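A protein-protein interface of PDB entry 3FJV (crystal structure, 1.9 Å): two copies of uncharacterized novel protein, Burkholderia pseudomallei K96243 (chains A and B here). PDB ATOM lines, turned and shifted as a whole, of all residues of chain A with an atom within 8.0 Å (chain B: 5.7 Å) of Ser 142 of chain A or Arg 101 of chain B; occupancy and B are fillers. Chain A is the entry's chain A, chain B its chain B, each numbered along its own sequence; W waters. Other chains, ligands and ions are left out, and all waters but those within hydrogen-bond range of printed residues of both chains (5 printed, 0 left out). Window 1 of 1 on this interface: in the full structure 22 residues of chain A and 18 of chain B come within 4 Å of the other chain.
The side-chain carboxylate of Asp 130 of chain A is in salt-bridge range of the guanidinium group of Arg 102 of chain B.
The side-chain carboxylate of Asp 130 of chain A sits at hydrogen-bond distance from a ring nitrogen (ND1) of His 145 of chain A. The backbone carbonyl oxygen (O) of Phe 146 of chain A lies within hydrogen-bond range of the backbone NH (N) of Asp 130 of chain A (2.8 Å). OG of Ser 142 of chain A lies within hydrogen-bond range of O of Val 144 of chain A (2.9 Å). The guanidinium group (NE) of Arg 101 of chain B is in hydrogen-bond range of the backbone carbonyl oxygen (O) of Ile 93 of chain B. OD1 of Asn 97 of chain B lies within hydrogen-bond range of OG1 of Thr 99 of chain B (3.0 Å). OD1 of Asn 97 of chain B is in hydrogen-bond range of N of Gln 100 of chain B, 3.0 Å away.
Among the printed residues, merely in contact across the chains: Met 58 of chain A with Gln 100 of chain B (3.5 Å), Met 58 of chain A with Ala 103 of chain B (3.9 Å), Tyr 77 of chain A with Gln 100 of chain B (3.6 Å), Tyr 77 of chain A with Ala 103 of chain B (3.4 Å), Gln 92 of chain A with Thr 99 of chain B (3.5 Å), Leu 133 of chain A with Arg 102 of chain B (3.6 Å), Ser 142 of chain A with Arg 101 of chain B (3.7 Å), Ala 143 of chain A with Glu 98 of chain B (3.3 Å), Val 144 of chain A with Glu 98 of chain B (3.7 Å), Val 144 of chain A with Arg 102 of chain B (3.5 Å) and Phe 146 of chain A with Arg 102 of chain B (3.6 Å).
Ser 142 of chain A touches one residue of chain B. Of chain A, only Ser 142 (3.7 Å) comes within 4 Å of Arg 101 of chain B. Of the printed residues of chain A, Glu 98 of chain B touches Ala 143 and Val 144. Printed residues of chain A within 4 Å of Gln 100 of chain B: Met 58 (3.5 Å) and Tyr 77 (3.6 Å). Of the printed residues of chain B, Gln 92 of chain A touches Thr 99 (3.5 Å). Of the printed residues of chain B, Leu 133 of chain A touches Arg 102 (3.6 Å). Of the printed residues of chain A, Ala 103 of chain B touches Met 58 (3.9 Å) and Tyr 77 (3.4 Å). The nearest residue of chain A that does not touch Arg 101 of chain B is Thr 141 of chain A (5.2 Å).
Of the 12 printed residues of chain B, 6 touch a printed residue of chain A. Printed residues of chain B that touch a printed residue of chain A: Glu 98, Thr 99, Gln 100, Arg 101, Arg 102 and Ala 103. Among the printed residues, 12 pairs touch across the chains. Among the printed residues, Asp or Glu carboxylates within 4 Å of a Lys or Arg side-chain nitrogen of the other chain: Asp 130 of chain A with Arg 102 of chain B (2.9 Å).
Positions printed for both chains: 93 and 105. Of the 12 pairs that touch across the chains among the printed residues, none has its exchanged pair printed and touching as well.
Water W1 bridges OE1 of Gln 92 of chain A and OE1 of Glu 98 of chain B. Water W2 lies within hydrogen-bond range of OG1 of Thr 99 of chain B (2.7 Å) and OH of Tyr 77 of chain A (2.7 Å). Water W5 bridges the backbone carbonyl oxygen of Thr 141 of chain A (2.7 Å) and the guanidinium group of Arg 101 of chain B (3.4 Å). Water W4 lies within hydrogen-bond range of N of Glu 98 of chain B (3.0 Å), N of Thr 99 of chain B (3.3 Å) and OE1 of Gln 92 of chain A (3.4 Å). Water W3 lies within hydrogen-bond range of NE of Arg 102 of chain B, O of Val 144 of chain A and ND1 of His 145 of chain A.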
ATOM      1  N   MET A  58     -16.300  -3.552   0.164  1.00  0.00           N
ATOM      2  CA  MET A  58     -16.514  -3.211  -1.223  1.00  0.00           C
ATOM      3  C   MET A  58     -17.175  -4.343  -2.011  1.00  0.00           C
ATOM      4  O   MET A  58     -18.160  -4.118  -2.719  1.00  0.00           O
ATOM      5  CB  MET A  58     -15.197  -2.848  -1.919  1.00  0.00           C
ATOM      6  CG  MET A  58     -15.358  -2.401  -3.434  1.00  0.00           C
ATOM      7  SD  MET A  58     -16.056  -0.661  -3.729  1.00  0.00           S
ATOM      8  CE  MET A  58     -14.383   0.359  -3.879  1.00  0.00           C
ATOM      9  N   TYR A  77      -6.800  -1.420  -3.689  1.00  0.00           N
ATOM     10  CA  TYR A  77      -6.425  -1.193  -2.298  1.00  0.00           C
ATOM     11  C   TYR A  77      -4.950  -1.473  -1.940  1.00  0.00           C
ATOM     12  O   TYR A  77      -4.532  -1.155  -0.828  1.00  0.00           O
ATOM     13  CB  TYR A  77      -7.367  -1.963  -1.344  1.00  0.00           C
ATOM     14  CG  TYR A  77      -8.762  -1.326  -1.220  1.00  0.00           C
ATOM     15  CD1 TYR A  77      -9.007  -0.324  -0.294  1.00  0.00           C
ATOM     16  CD2 TYR A  77      -9.823  -1.733  -2.031  1.00  0.00           C
ATOM     17  CE1 TYR A  77     -10.272   0.240  -0.161  1.00  0.00           C
ATOM     18  CE2 TYR A  77     -11.054  -1.197  -1.909  1.00  0.00           C
ATOM     19  CZ  TYR A  77     -11.294  -0.207  -0.951  1.00  0.00           C
ATOM     20  OH  TYR A  77     -12.528   0.388  -0.826  1.00  0.00           O
ATOM     21  N   LEU A  91      -6.055   9.460   4.733  1.00  0.00           N
ATOM     22  CA  LEU A  91      -6.347  10.776   5.285  1.00  0.00           C
ATOM     23  C   LEU A  91      -7.751  11.171   4.833  1.00  0.00           C
ATOM     24  O   LEU A  91      -8.071  11.121   3.637  1.00  0.00           O
ATOM     25  CB  LEU A  91      -5.353  11.830   4.792  1.00  0.00           C
ATOM     26  CG  LEU A  91      -5.551  13.315   5.195  1.00  0.00           C
ATOM     27  CD1 LEU A  91      -5.287  13.632   6.649  1.00  0.00           C
ATOM     28  CD2 LEU A  91      -4.626  14.238   4.366  1.00  0.00           C
ATOM     29  N   GLN A  92      -8.560  11.607   5.790  1.00  0.00           N
ATOM     30  CA  GLN A  92      -9.902  12.101   5.481  1.00  0.00           C
ATOM     31  C   GLN A  92     -10.030  13.505   6.013  1.00  0.00           C
ATOM     32  O   GLN A  92      -9.590  13.797   7.111  1.00  0.00           O
ATOM     33  CB  GLN A  92     -10.989  11.202   6.058  1.00  0.00           C
ATOM     34  CG  GLN A  92     -11.026   9.828   5.361  1.00  0.00           C
ATOM     35  CD  GLN A  92     -12.342   9.100   5.554  1.00  0.00           C
ATOM     36  OE1 GLN A  92     -13.404   9.590   5.107  1.00  0.00           O
ATOM     37  NE2 GLN A  92     -12.289   7.920   6.177  1.00  0.00           N
ATOM     38  N   ILE A  93     -10.607  14.372   5.193  1.00  0.00           N
ATOM     39  CA  ILE A  93     -10.873  15.768   5.526  1.00  0.00           C
ATOM     40  C   ILE A  93     -12.379  15.819   5.706  1.00  0.00           C
ATOM     41  O   ILE A  93     -13.109  15.453   4.776  1.00  0.00           O
ATOM     42  CB  ILE A  93     -10.439  16.680   4.352  1.00  0.00           C
ATOM     43  CG1 ILE A  93      -8.946  16.508   4.075  1.00  0.00           C
ATOM     44  CG2 ILE A  93     -10.711  18.177   4.655  1.00  0.00           C
ATOM     45  CD1 ILE A  93      -8.536  16.990   2.664  1.00  0.00           C
ATOM     46  N   LEU A 105     -11.952  22.350   0.874  1.00  0.00           N
ATOM     47  CA  LEU A 105     -11.147  21.576  -0.079  1.00  0.00           C
ATOM     48  C   LEU A 105     -10.338  22.489  -1.017  1.00  0.00           C
ATOM     49  O   LEU A 105      -9.184  22.182  -1.339  1.00  0.00           O
ATOM     50  CB  LEU A 105     -12.048  20.604  -0.868  1.00  0.00           C
ATOM     51  CG  LEU A 105     -12.611  19.448  -0.012  1.00  0.00           C
ATOM     52  CD1 LEU A 105     -13.541  18.551  -0.846  1.00  0.00           C
ATOM     53  CD2 LEU A 105     -11.472  18.626   0.633  1.00  0.00           C
ATOM     54  N   ALA A 106     -10.908  23.632  -1.397  1.00  0.00           N
ATOM     55  CA  ALA A 106     -10.163  24.625  -2.180  1.00  0.00           C
ATOM     56  C   ALA A 106      -9.042  25.266  -1.387  1.00  0.00           C
ATOM     57  O   ALA A 106      -7.892  25.369  -1.861  1.00  0.00           O
ATOM     58  CB  ALA A 106     -11.117  25.734  -2.733  1.00  0.00           C
ATOM     59  N   LEU A 108      -7.574  24.187   1.198  1.00  0.00           N
ATOM     60  CA  LEU A 108      -6.629  23.162   1.670  1.00  0.00           C
ATOM     61  C   LEU A 108      -5.929  22.399   0.562  1.00  0.00           C
ATOM     62  O   LEU A 108      -5.259  21.397   0.817  1.00  0.00           O
ATOM     63  CB  LEU A 108      -7.360  22.191   2.586  1.00  0.00           C
ATOM     64  CG  LEU A 108      -7.886  22.806   3.890  1.00  0.00           C
ATOM     65  CD1 LEU A 108      -8.482  21.725   4.739  1.00  0.00           C
ATOM     66  CD2 LEU A 108      -6.835  23.542   4.660  1.00  0.00           C
ATOM     67  N   VAL A 109      -6.017  22.883  -0.678  1.00  0.00           N
ATOM     68  CA  VAL A 109      -5.317  22.212  -1.775  1.00  0.00           C
ATOM     69  C   VAL A 109      -3.854  21.911  -1.392  1.00  0.00           C
ATOM     70  O   VAL A 109      -3.138  22.739  -0.825  1.00  0.00           O
ATOM     71  CB  VAL A 109      -5.360  23.056  -3.070  1.00  0.00           C
ATOM     72  CG1 VAL A 109      -4.733  24.396  -2.814  1.00  0.00           C
ATOM     73  CG2 VAL A 109      -4.670  22.316  -4.207  1.00  0.00           C
ATOM     74  N   ILE A 111      -2.806  19.922   0.915  1.00  0.00           N
ATOM     75  CA  ILE A 111      -2.595  19.536   2.338  1.00  0.00           C
ATOM     76  C   ILE A 111      -2.057  18.122   2.522  1.00  0.00           C
ATOM     77  O   ILE A 111      -1.284  17.855   3.439  1.00  0.00           O
ATOM     78  CB  ILE A 111      -3.880  19.739   3.189  1.00  0.00           C
ATOM     79  CG1 ILE A 111      -3.522  19.732   4.671  1.00  0.00           C
ATOM     80  CG2 ILE A 111      -4.981  18.707   2.848  1.00  0.00           C
ATOM     81  CD1 ILE A 111      -4.644  20.241   5.583  1.00  0.00           C
ATOM     82  N   GLU A 112      -2.448  17.208   1.651  1.00  0.00           N
ATOM     83  CA  GLU A 112      -1.966  15.827   1.725  1.00  0.00           C
ATOM     84  C   GLU A 112      -0.446  15.676   1.615  1.00  0.00           C
ATOM     85  O   GLU A 112       0.090  14.654   2.008  1.00  0.00           O
ATOM     86  CB  GLU A 112      -2.656  14.958   0.684  1.00  0.00           C
ATOM     87  CG  GLU A 112      -2.295  15.239  -0.790  1.00  0.00           C
ATOM     88  CD  GLU A 112      -3.053  16.441  -1.392  1.00  0.00           C
ATOM     89  OE1 GLU A 112      -3.697  17.183  -0.644  1.00  0.00           O
ATOM     90  OE2 GLU A 112      -3.004  16.636  -2.612  1.00  0.00           O
ATOM     91  N   ASP A 130      -1.018   9.803  -2.843  1.00  0.00           N
ATOM     92  CA  ASP A 130      -1.824   9.557  -4.058  1.00  0.00           C
ATOM     93  C   ASP A 130      -0.992   9.126  -5.265  1.00  0.00           C
ATOM     94  O   ASP A 130      -1.314   9.460  -6.413  1.00  0.00           O
ATOM     95  CB  ASP A 130      -2.704  10.807  -4.388  1.00  0.00           C
ATOM     96  CG  ASP A 130      -3.546  11.272  -3.196  1.00  0.00           C
ATOM     97  OD1 ASP A 130      -4.110  10.391  -2.474  1.00  0.00           O
ATOM     98  OD2 ASP A 130      -3.637  12.514  -3.002  1.00  0.00           O
ATOM     99  N   LEU A 133      -2.660   7.591  -8.329  1.00  0.00           N
ATOM    100  CA  LEU A 133      -3.490   8.338  -9.224  1.00  0.00           C
ATOM    101  C   LEU A 133      -2.614   9.047 -10.234  1.00  0.00           C
ATOM    102  O   LEU A 133      -1.600   9.701  -9.872  1.00  0.00           O
ATOM    103  CB  LEU A 133      -4.335   9.364  -8.481  1.00  0.00           C
ATOM    104  CG  LEU A 133      -5.389   8.799  -7.499  1.00  0.00           C
ATOM    105  CD1 LEU A 133      -6.124   9.969  -6.923  1.00  0.00           C
ATOM    106  CD2 LEU A 133      -6.313   7.802  -8.235  1.00  0.00           C
ATOM    107  N   THR A 137      -5.701  13.082 -12.324  1.00  0.00           N
ATOM    108  CA  THR A 137      -6.615  12.627 -11.271  1.00  0.00           C
ATOM    109  C   THR A 137      -6.122  13.133  -9.923  1.00  0.00           C
ATOM    110  O   THR A 137      -6.912  13.633  -9.122  1.00  0.00           O
ATOM    111  CB  THR A 137      -6.718  11.082 -11.208  1.00  0.00           C
ATOM    112  OG1 THR A 137      -6.900  10.548 -12.524  1.00  0.00           O
ATOM    113  CG2 THR A 137      -7.885  10.655 -10.315  1.00  0.00           C
ATOM    114  N   ALA A 138      -4.811  12.997  -9.690  1.00  0.00           N
ATOM    115  CA  ALA A 138      -4.183  13.427  -8.435  1.00  0.00           C
ATOM    116  C   ALA A 138      -4.374  14.923  -8.184  1.00  0.00           C
ATOM    117  O   ALA A 138      -4.450  15.350  -7.037  1.00  0.00           O
ATOM    118  CB  ALA A 138      -2.672  13.070  -8.419  1.00  0.00           C
ATOM    119  N   GLU A 139      -4.448  15.712  -9.258  1.00  0.00           N
ATOM    120  CA  GLU A 139      -4.595  17.160  -9.143  1.00  0.00           C
ATOM    121  C   GLU A 139      -6.030  17.598  -8.735  1.00  0.00           C
ATOM    122  O   GLU A 139      -6.221  18.692  -8.187  1.00  0.00           O
ATOM    123  CB  GLU A 139      -4.182  17.806 -10.464  1.00  0.00           C
ATOM    124  CG  GLU A 139      -3.817  19.273 -10.349  1.00  0.00           C
ATOM    125  CD  GLU A 139      -3.936  20.009 -11.671  1.00  0.00           C
ATOM    126  OE1 GLU A 139      -4.708  19.568 -12.551  1.00  0.00           O
ATOM    127  OE2 GLU A 139      -3.264  21.046 -11.824  1.00  0.00           O
ATOM    128  N   LYS A 140      -7.034  16.763  -9.015  1.00  0.00           N
ATOM    129  CA  LYS A 140      -8.402  17.003  -8.525  1.00  0.00           C
ATOM    130  C   LYS A 140      -8.440  16.812  -7.007  1.00  0.00           C
ATOM    131  O   LYS A 140      -7.903  15.826  -6.510  1.00  0.00           O
ATOM    132  CB  LYS A 140      -9.392  16.051  -9.202  1.00  0.00           C
ATOM    133  CG  LYS A 140      -9.913  16.594 -10.529  1.00  0.00           C
ATOM    134  CD  LYS A 140     -10.551  15.531 -11.402  1.00  0.00           C
ATOM    135  CE  LYS A 140      -9.602  15.021 -12.474  1.00  0.00           C
ATOM    136  NZ  LYS A 140     -10.363  14.504 -13.654  1.00  0.00           N
ATOM    137  N   THR A 141      -9.051  17.751  -6.272  1.00  0.00           N
ATOM    138  CA  THR A 141      -9.142  17.632  -4.804  1.00  0.00           C
ATOM    139  C   THR A 141     -10.053  16.435  -4.406  1.00  0.00           C
ATOM    140  O   THR A 141     -10.785  15.847  -5.233  1.00  0.00           O
ATOM    141  CB  THR A 141      -9.575  18.981  -4.062  1.00  0.00           C
ATOM    142  OG1 THR A 141     -10.886  19.391  -4.481  1.00  0.00           O
ATOM    143  CG2 THR A 141      -8.546  20.145  -4.282  1.00  0.00           C
ATOM    144  N   SER A 142      -9.972  16.056  -3.135  1.00  0.00           N
ATOM    145  CA  SER A 142     -10.671  14.881  -2.664  1.00  0.00           C
ATOM    146  C   SER A 142     -10.672  15.056  -1.153  1.00  0.00           C
ATOM    147  O   SER A 142      -9.743  15.608  -0.583  1.00  0.00           O
ATOM    148  CB  SER A 142      -9.947  13.594  -3.146  1.00  0.00           C
ATOM    149  OG  SER A 142     -10.612  12.378  -2.756  1.00  0.00           O
ATOM    150  N   ALA A 143     -11.755  14.670  -0.511  1.00  0.00           N
ATOM    151  CA  ALA A 143     -11.771  14.616   0.938  1.00  0.00           C
ATOM    152  C   ALA A 143     -10.966  13.401   1.411  1.00  0.00           C
ATOM    153  O   ALA A 143     -10.853  13.194   2.626  1.00  0.00           O
ATOM    154  CB  ALA A 143     -13.226  14.543   1.458  1.00  0.00           C
ATOM    155  N   VAL A 144     -10.498  12.546   0.484  1.00  0.00           N
ATOM    156  CA  VAL A 144      -9.786  11.289   0.868  1.00  0.00           C
ATOM    157  C   VAL A 144      -8.472  11.144   0.097  1.00  0.00           C
ATOM    158  O   VAL A 144      -8.463  11.210  -1.113  1.00  0.00           O
ATOM    159  CB  VAL A 144     -10.644  10.038   0.695  1.00  0.00           C
ATOM    160  CG1 VAL A 144      -9.898   8.769   1.170  1.00  0.00           C
ATOM    161  CG2 VAL A 144     -11.964  10.174   1.481  1.00  0.00           C
ATOM    162  N   HIS A 145      -7.369  10.907   0.809  1.00  0.00           N
ATOM    163  CA  HIS A 145      -6.059  10.731   0.182  1.00  0.00           C
ATOM    164  C   HIS A 145      -5.383   9.491   0.758  1.00  0.00           C
ATOM    165  O   HIS A 145      -5.657   9.107   1.886  1.00  0.00           O
ATOM    166  CB  HIS A 145      -5.203  11.956   0.481  1.00  0.00           C
ATOM    167  CG  HIS A 145      -5.736  13.212  -0.131  1.00  0.00           C
ATOM    168  ND1 HIS A 145      -5.391  13.617  -1.404  1.00  0.00           N
ATOM    169  CD2 HIS A 145      -6.589  14.156   0.351  1.00  0.00           C
ATOM    170  CE1 HIS A 145      -6.021  14.750  -1.686  1.00  0.00           C
ATOM    171  NE2 HIS A 145      -6.733  15.111  -0.629  1.00  0.00           N
ATOM    172  N   PHE A 146      -4.550   8.846  -0.042  1.00  0.00           N
ATOM    173  CA  PHE A 146      -3.762   7.685   0.392  1.00  0.00           C
ATOM    174  C   PHE A 146      -2.327   8.154   0.594  1.00  0.00           C
ATOM    175  O   PHE A 146      -1.699   8.702  -0.341  1.00  0.00           O
ATOM    176  CB  PHE A 146      -3.839   6.604  -0.684  1.00  0.00           C
ATOM    177  CG  PHE A 146      -5.190   5.911  -0.812  1.00  0.00           C
ATOM    178  CD1 PHE A 146      -6.217   6.072   0.116  1.00  0.00           C
ATOM    179  CD2 PHE A 146      -5.401   5.009  -1.879  1.00  0.00           C
ATOM    180  CE1 PHE A 146      -7.425   5.413  -0.013  1.00  0.00           C
ATOM    181  CE2 PHE A 146      -6.623   4.347  -2.013  1.00  0.00           C
ATOM    182  CZ  PHE A 146      -7.640   4.561  -1.045  1.00  0.00           C
ATOM    183  N   ILE B  93     -18.912  11.452  -8.693  1.00  0.00           N
ATOM    184  CA  ILE B  93     -18.713  10.025  -8.590  1.00  0.00           C
ATOM    185  C   ILE B  93     -19.074   9.723  -7.164  1.00  0.00           C
ATOM    186  O   ILE B  93     -18.582  10.377  -6.253  1.00  0.00           O
ATOM    187  CB  ILE B  93     -17.282   9.645  -8.846  1.00  0.00           C
ATOM    188  CG1 ILE B  93     -16.915   9.976 -10.305  1.00  0.00           C
ATOM    189  CG2 ILE B  93     -17.030   8.123  -8.530  1.00  0.00           C
ATOM    190  CD1 ILE B  93     -15.474   9.703 -10.634  1.00  0.00           C
ATOM    191  N   GLU B  94     -19.940   8.758  -6.967  1.00  0.00           N
ATOM    192  CA  GLU B  94     -20.465   8.495  -5.655  1.00  0.00           C
ATOM    193  C   GLU B  94     -20.554   6.997  -5.326  1.00  0.00           C
ATOM    194  O   GLU B  94     -21.079   6.200  -6.105  1.00  0.00           O
ATOM    195  CB  GLU B  94     -21.833   9.127  -5.550  1.00  0.00           C
ATOM    196  CG  GLU B  94     -22.351   9.154  -4.132  1.00  0.00           C
ATOM    197  CD  GLU B  94     -23.702   9.847  -4.023  1.00  0.00           C
ATOM    198  OE1 GLU B  94     -24.047  10.654  -4.915  1.00  0.00           O
ATOM    199  OE2 GLU B  94     -24.411   9.565  -3.044  1.00  0.00           O
ATOM    200  N   TYR B  95     -19.988   6.640  -4.166  1.00  0.00           N
ATOM    201  CA  TYR B  95     -20.009   5.294  -3.653  1.00  0.00           C
ATOM    202  C   TYR B  95     -20.637   5.330  -2.274  1.00  0.00           C
ATOM    203  O   TYR B  95     -20.936   6.414  -1.741  1.00  0.00           O
ATOM    204  CB  TYR B  95     -18.578   4.674  -3.620  1.00  0.00           C
ATOM    205  CG  TYR B  95     -18.149   4.236  -4.995  1.00  0.00           C
ATOM    206  CD1 TYR B  95     -17.799   5.183  -5.981  1.00  0.00           C
ATOM    207  CD2 TYR B  95     -18.022   2.878  -5.312  1.00  0.00           C
ATOM    208  CE1 TYR B  95     -17.414   4.763  -7.256  1.00  0.00           C
ATOM    209  CE2 TYR B  95     -17.628   2.468  -6.560  1.00  0.00           C
ATOM    210  CZ  TYR B  95     -17.339   3.405  -7.515  1.00  0.00           C
ATOM    211  OH  TYR B  95     -16.979   2.961  -8.751  1.00  0.00           O
ATOM    212  N   ASN B  97     -19.409   4.977   0.595  1.00  0.00           N
ATOM    213  CA  ASN B  97     -18.677   5.955   1.381  1.00  0.00           C
ATOM    214  C   ASN B  97     -17.489   6.506   0.577  1.00  0.00           C
ATOM    215  O   ASN B  97     -17.192   6.036  -0.503  1.00  0.00           O
ATOM    216  CB  ASN B  97     -18.220   5.348   2.699  1.00  0.00           C
ATOM    217  CG  ASN B  97     -17.287   4.201   2.505  1.00  0.00           C
ATOM    218  OD1 ASN B  97     -16.329   4.298   1.775  1.00  0.00           O
ATOM    219  ND2 ASN B  97     -17.519   3.135   3.218  1.00  0.00           N
ATOM    220  N   GLU B  98     -16.785   7.449   1.166  1.00  0.00           N
ATOM    221  CA  GLU B  98     -15.798   8.200   0.436  1.00  0.00           C
ATOM    222  C   GLU B  98     -14.484   7.437   0.223  1.00  0.00           C
ATOM    223  O   GLU B  98     -13.763   7.726  -0.707  1.00  0.00           O
ATOM    224  CB  GLU B  98     -15.549   9.500   1.145  1.00  0.00           C
ATOM    225  CG  GLU B  98     -16.799  10.391   1.131  1.00  0.00           C
ATOM    226  CD  GLU B  98     -16.444  11.836   0.992  1.00  0.00           C
ATOM    227  OE1 GLU B  98     -15.632  12.313   1.810  1.00  0.00           O
ATOM    228  OE2 GLU B  98     -16.959  12.480   0.050  1.00  0.00           O
ATOM    229  N   THR B  99     -14.186   6.477   1.085  1.00  0.00           N
ATOM    230  CA  THR B  99     -12.947   5.703   0.903  1.00  0.00           C
ATOM    231  C   THR B  99     -13.115   4.775  -0.294  1.00  0.00           C
ATOM    232  O   THR B  99     -12.179   4.572  -1.016  1.00  0.00           O
ATOM    233  CB  THR B  99     -12.494   4.962   2.150  1.00  0.00           C
ATOM    234  OG1 THR B  99     -13.497   4.008   2.559  1.00  0.00           O
ATOM    235  CG2 THR B  99     -12.179   5.988   3.291  1.00  0.00           C
ATOM    236  N   GLN B 100     -14.308   4.232  -0.500  1.00  0.00           N
ATOM    237  CA  GLN B 100     -14.572   3.406  -1.688  1.00  0.00           C
ATOM    238  C   GLN B 100     -14.538   4.252  -2.937  1.00  0.00           C
ATOM    239  O   GLN B 100     -13.964   3.849  -3.955  1.00  0.00           O
ATOM    240  CB  GLN B 100     -15.917   2.650  -1.556  1.00  0.00           C
ATOM    241  CG  GLN B 100     -15.932   1.629  -0.479  1.00  0.00           C
ATOM    242  CD  GLN B 100     -17.317   1.011  -0.245  1.00  0.00           C
ATOM    243  OE1 GLN B 100     -18.302   1.513  -0.766  1.00  0.00           O
ATOM    244  NE2 GLN B 100     -17.383  -0.070   0.550  1.00  0.00           N
ATOM    245  N   ARG B 101     -15.097   5.458  -2.858  1.00  0.00           N
ATOM    246  CA  ARG B 101     -14.981   6.338  -3.968  1.00  0.00           C
ATOM    247  C   ARG B 101     -13.494   6.508  -4.334  1.00  0.00           C
ATOM    248  O   ARG B 101     -13.123   6.382  -5.472  1.00  0.00           O
ATOM    249  CB  ARG B 101     -15.642   7.697  -3.691  1.00  0.00           C
ATOM    250  CG  ARG B 101     -15.475   8.705  -4.812  1.00  0.00           C
ATOM    251  CD  ARG B 101     -15.967  10.100  -4.371  1.00  0.00           C
ATOM    252  NE  ARG B 101     -15.757  11.068  -5.423  1.00  0.00           N
ATOM    253  CZ  ARG B 101     -14.611  11.694  -5.645  1.00  0.00           C
ATOM    254  NH1 ARG B 101     -13.551  11.490  -4.871  1.00  0.00           N
ATOM    255  NH2 ARG B 101     -14.523  12.535  -6.659  1.00  0.00           N
ATOM    256  N   ARG B 102     -12.633   6.771  -3.355  1.00  0.00           N
ATOM    257  CA  ARG B 102     -11.224   7.043  -3.660  1.00  0.00           C
ATOM    258  C   ARG B 102     -10.531   5.810  -4.254  1.00  0.00           C
ATOM    259  O   ARG B 102      -9.638   5.919  -5.094  1.00  0.00           O
ATOM    260  CB  ARG B 102     -10.508   7.494  -2.363  1.00  0.00           C
ATOM    261  CG  ARG B 102      -9.020   7.648  -2.454  1.00  0.00           C
ATOM    262  CD  ARG B 102      -8.622   8.651  -3.552  1.00  0.00           C
ATOM    263  NE  ARG B 102      -7.166   8.779  -3.554  1.00  0.00           N
ATOM    264  CZ  ARG B 102      -6.322   7.868  -4.030  1.00  0.00           C
ATOM    265  NH1 ARG B 102      -6.754   6.783  -4.647  1.00  0.00           N
ATOM    266  NH2 ARG B 102      -5.034   8.081  -3.948  1.00  0.00           N
ATOM    267  N   ALA B 103     -10.943   4.624  -3.781  1.00  0.00           N
ATOM    268  CA  ALA B 103     -10.451   3.334  -4.274  1.00  0.00           C
ATOM    269  C   ALA B 103     -10.888   3.028  -5.720  1.00  0.00           C
ATOM    270  O   ALA B 103     -10.329   2.130  -6.325  1.00  0.00           O
ATOM    271  CB  ALA B 103     -10.944   2.148  -3.342  1.00  0.00           C
ATOM    272  N   ALA B 104     -11.927   3.704  -6.207  1.00  0.00           N
ATOM    273  CA  ALA B 104     -12.488   3.535  -7.580  1.00  0.00           C
ATOM    274  C   ALA B 104     -11.879   4.503  -8.617  1.00  0.00           C
ATOM    275  O   ALA B 104     -11.954   4.223  -9.833  1.00  0.00           O
ATOM    276  CB  ALA B 104     -14.076   3.733  -7.567  1.00  0.00           C
ATOM    277  N   LEU B 105     -11.306   5.625  -8.161  1.00  0.00           N
ATOM    278  CA  LEU B 105     -10.930   6.750  -9.034  1.00  0.00           C
ATOM    279  C   LEU B 105      -9.940   6.387 -10.139  1.00  0.00           C
ATOM    280  O   LEU B 105     -10.108   6.808 -11.307  1.00  0.00           O
ATOM    281  CB  LEU B 105     -10.412   7.947  -8.235  1.00  0.00           C
ATOM    282  CG  LEU B 105     -11.347   8.714  -7.282  1.00  0.00           C
ATOM    283  CD1 LEU B 105     -10.670   9.968  -6.802  1.00  0.00           C
ATOM    284  CD2 LEU B 105     -12.639   9.091  -7.960  1.00  0.00           C
HETATM  285  O   HOH W   1     -13.956  11.949   3.979  1.00  0.00           O
HETATM  286  O   HOH W   2     -12.875   1.559   1.601  1.00  0.00           O
HETATM  287  O   HOH W   3      -6.997  11.880  -3.875  1.00  0.00           O
HETATM  288  O   HOH W   4     -15.591   7.311   3.914  1.00  0.00           O
HETATM  289  O   HOH W   5     -11.261  13.459  -6.412  1.00  0.00           O
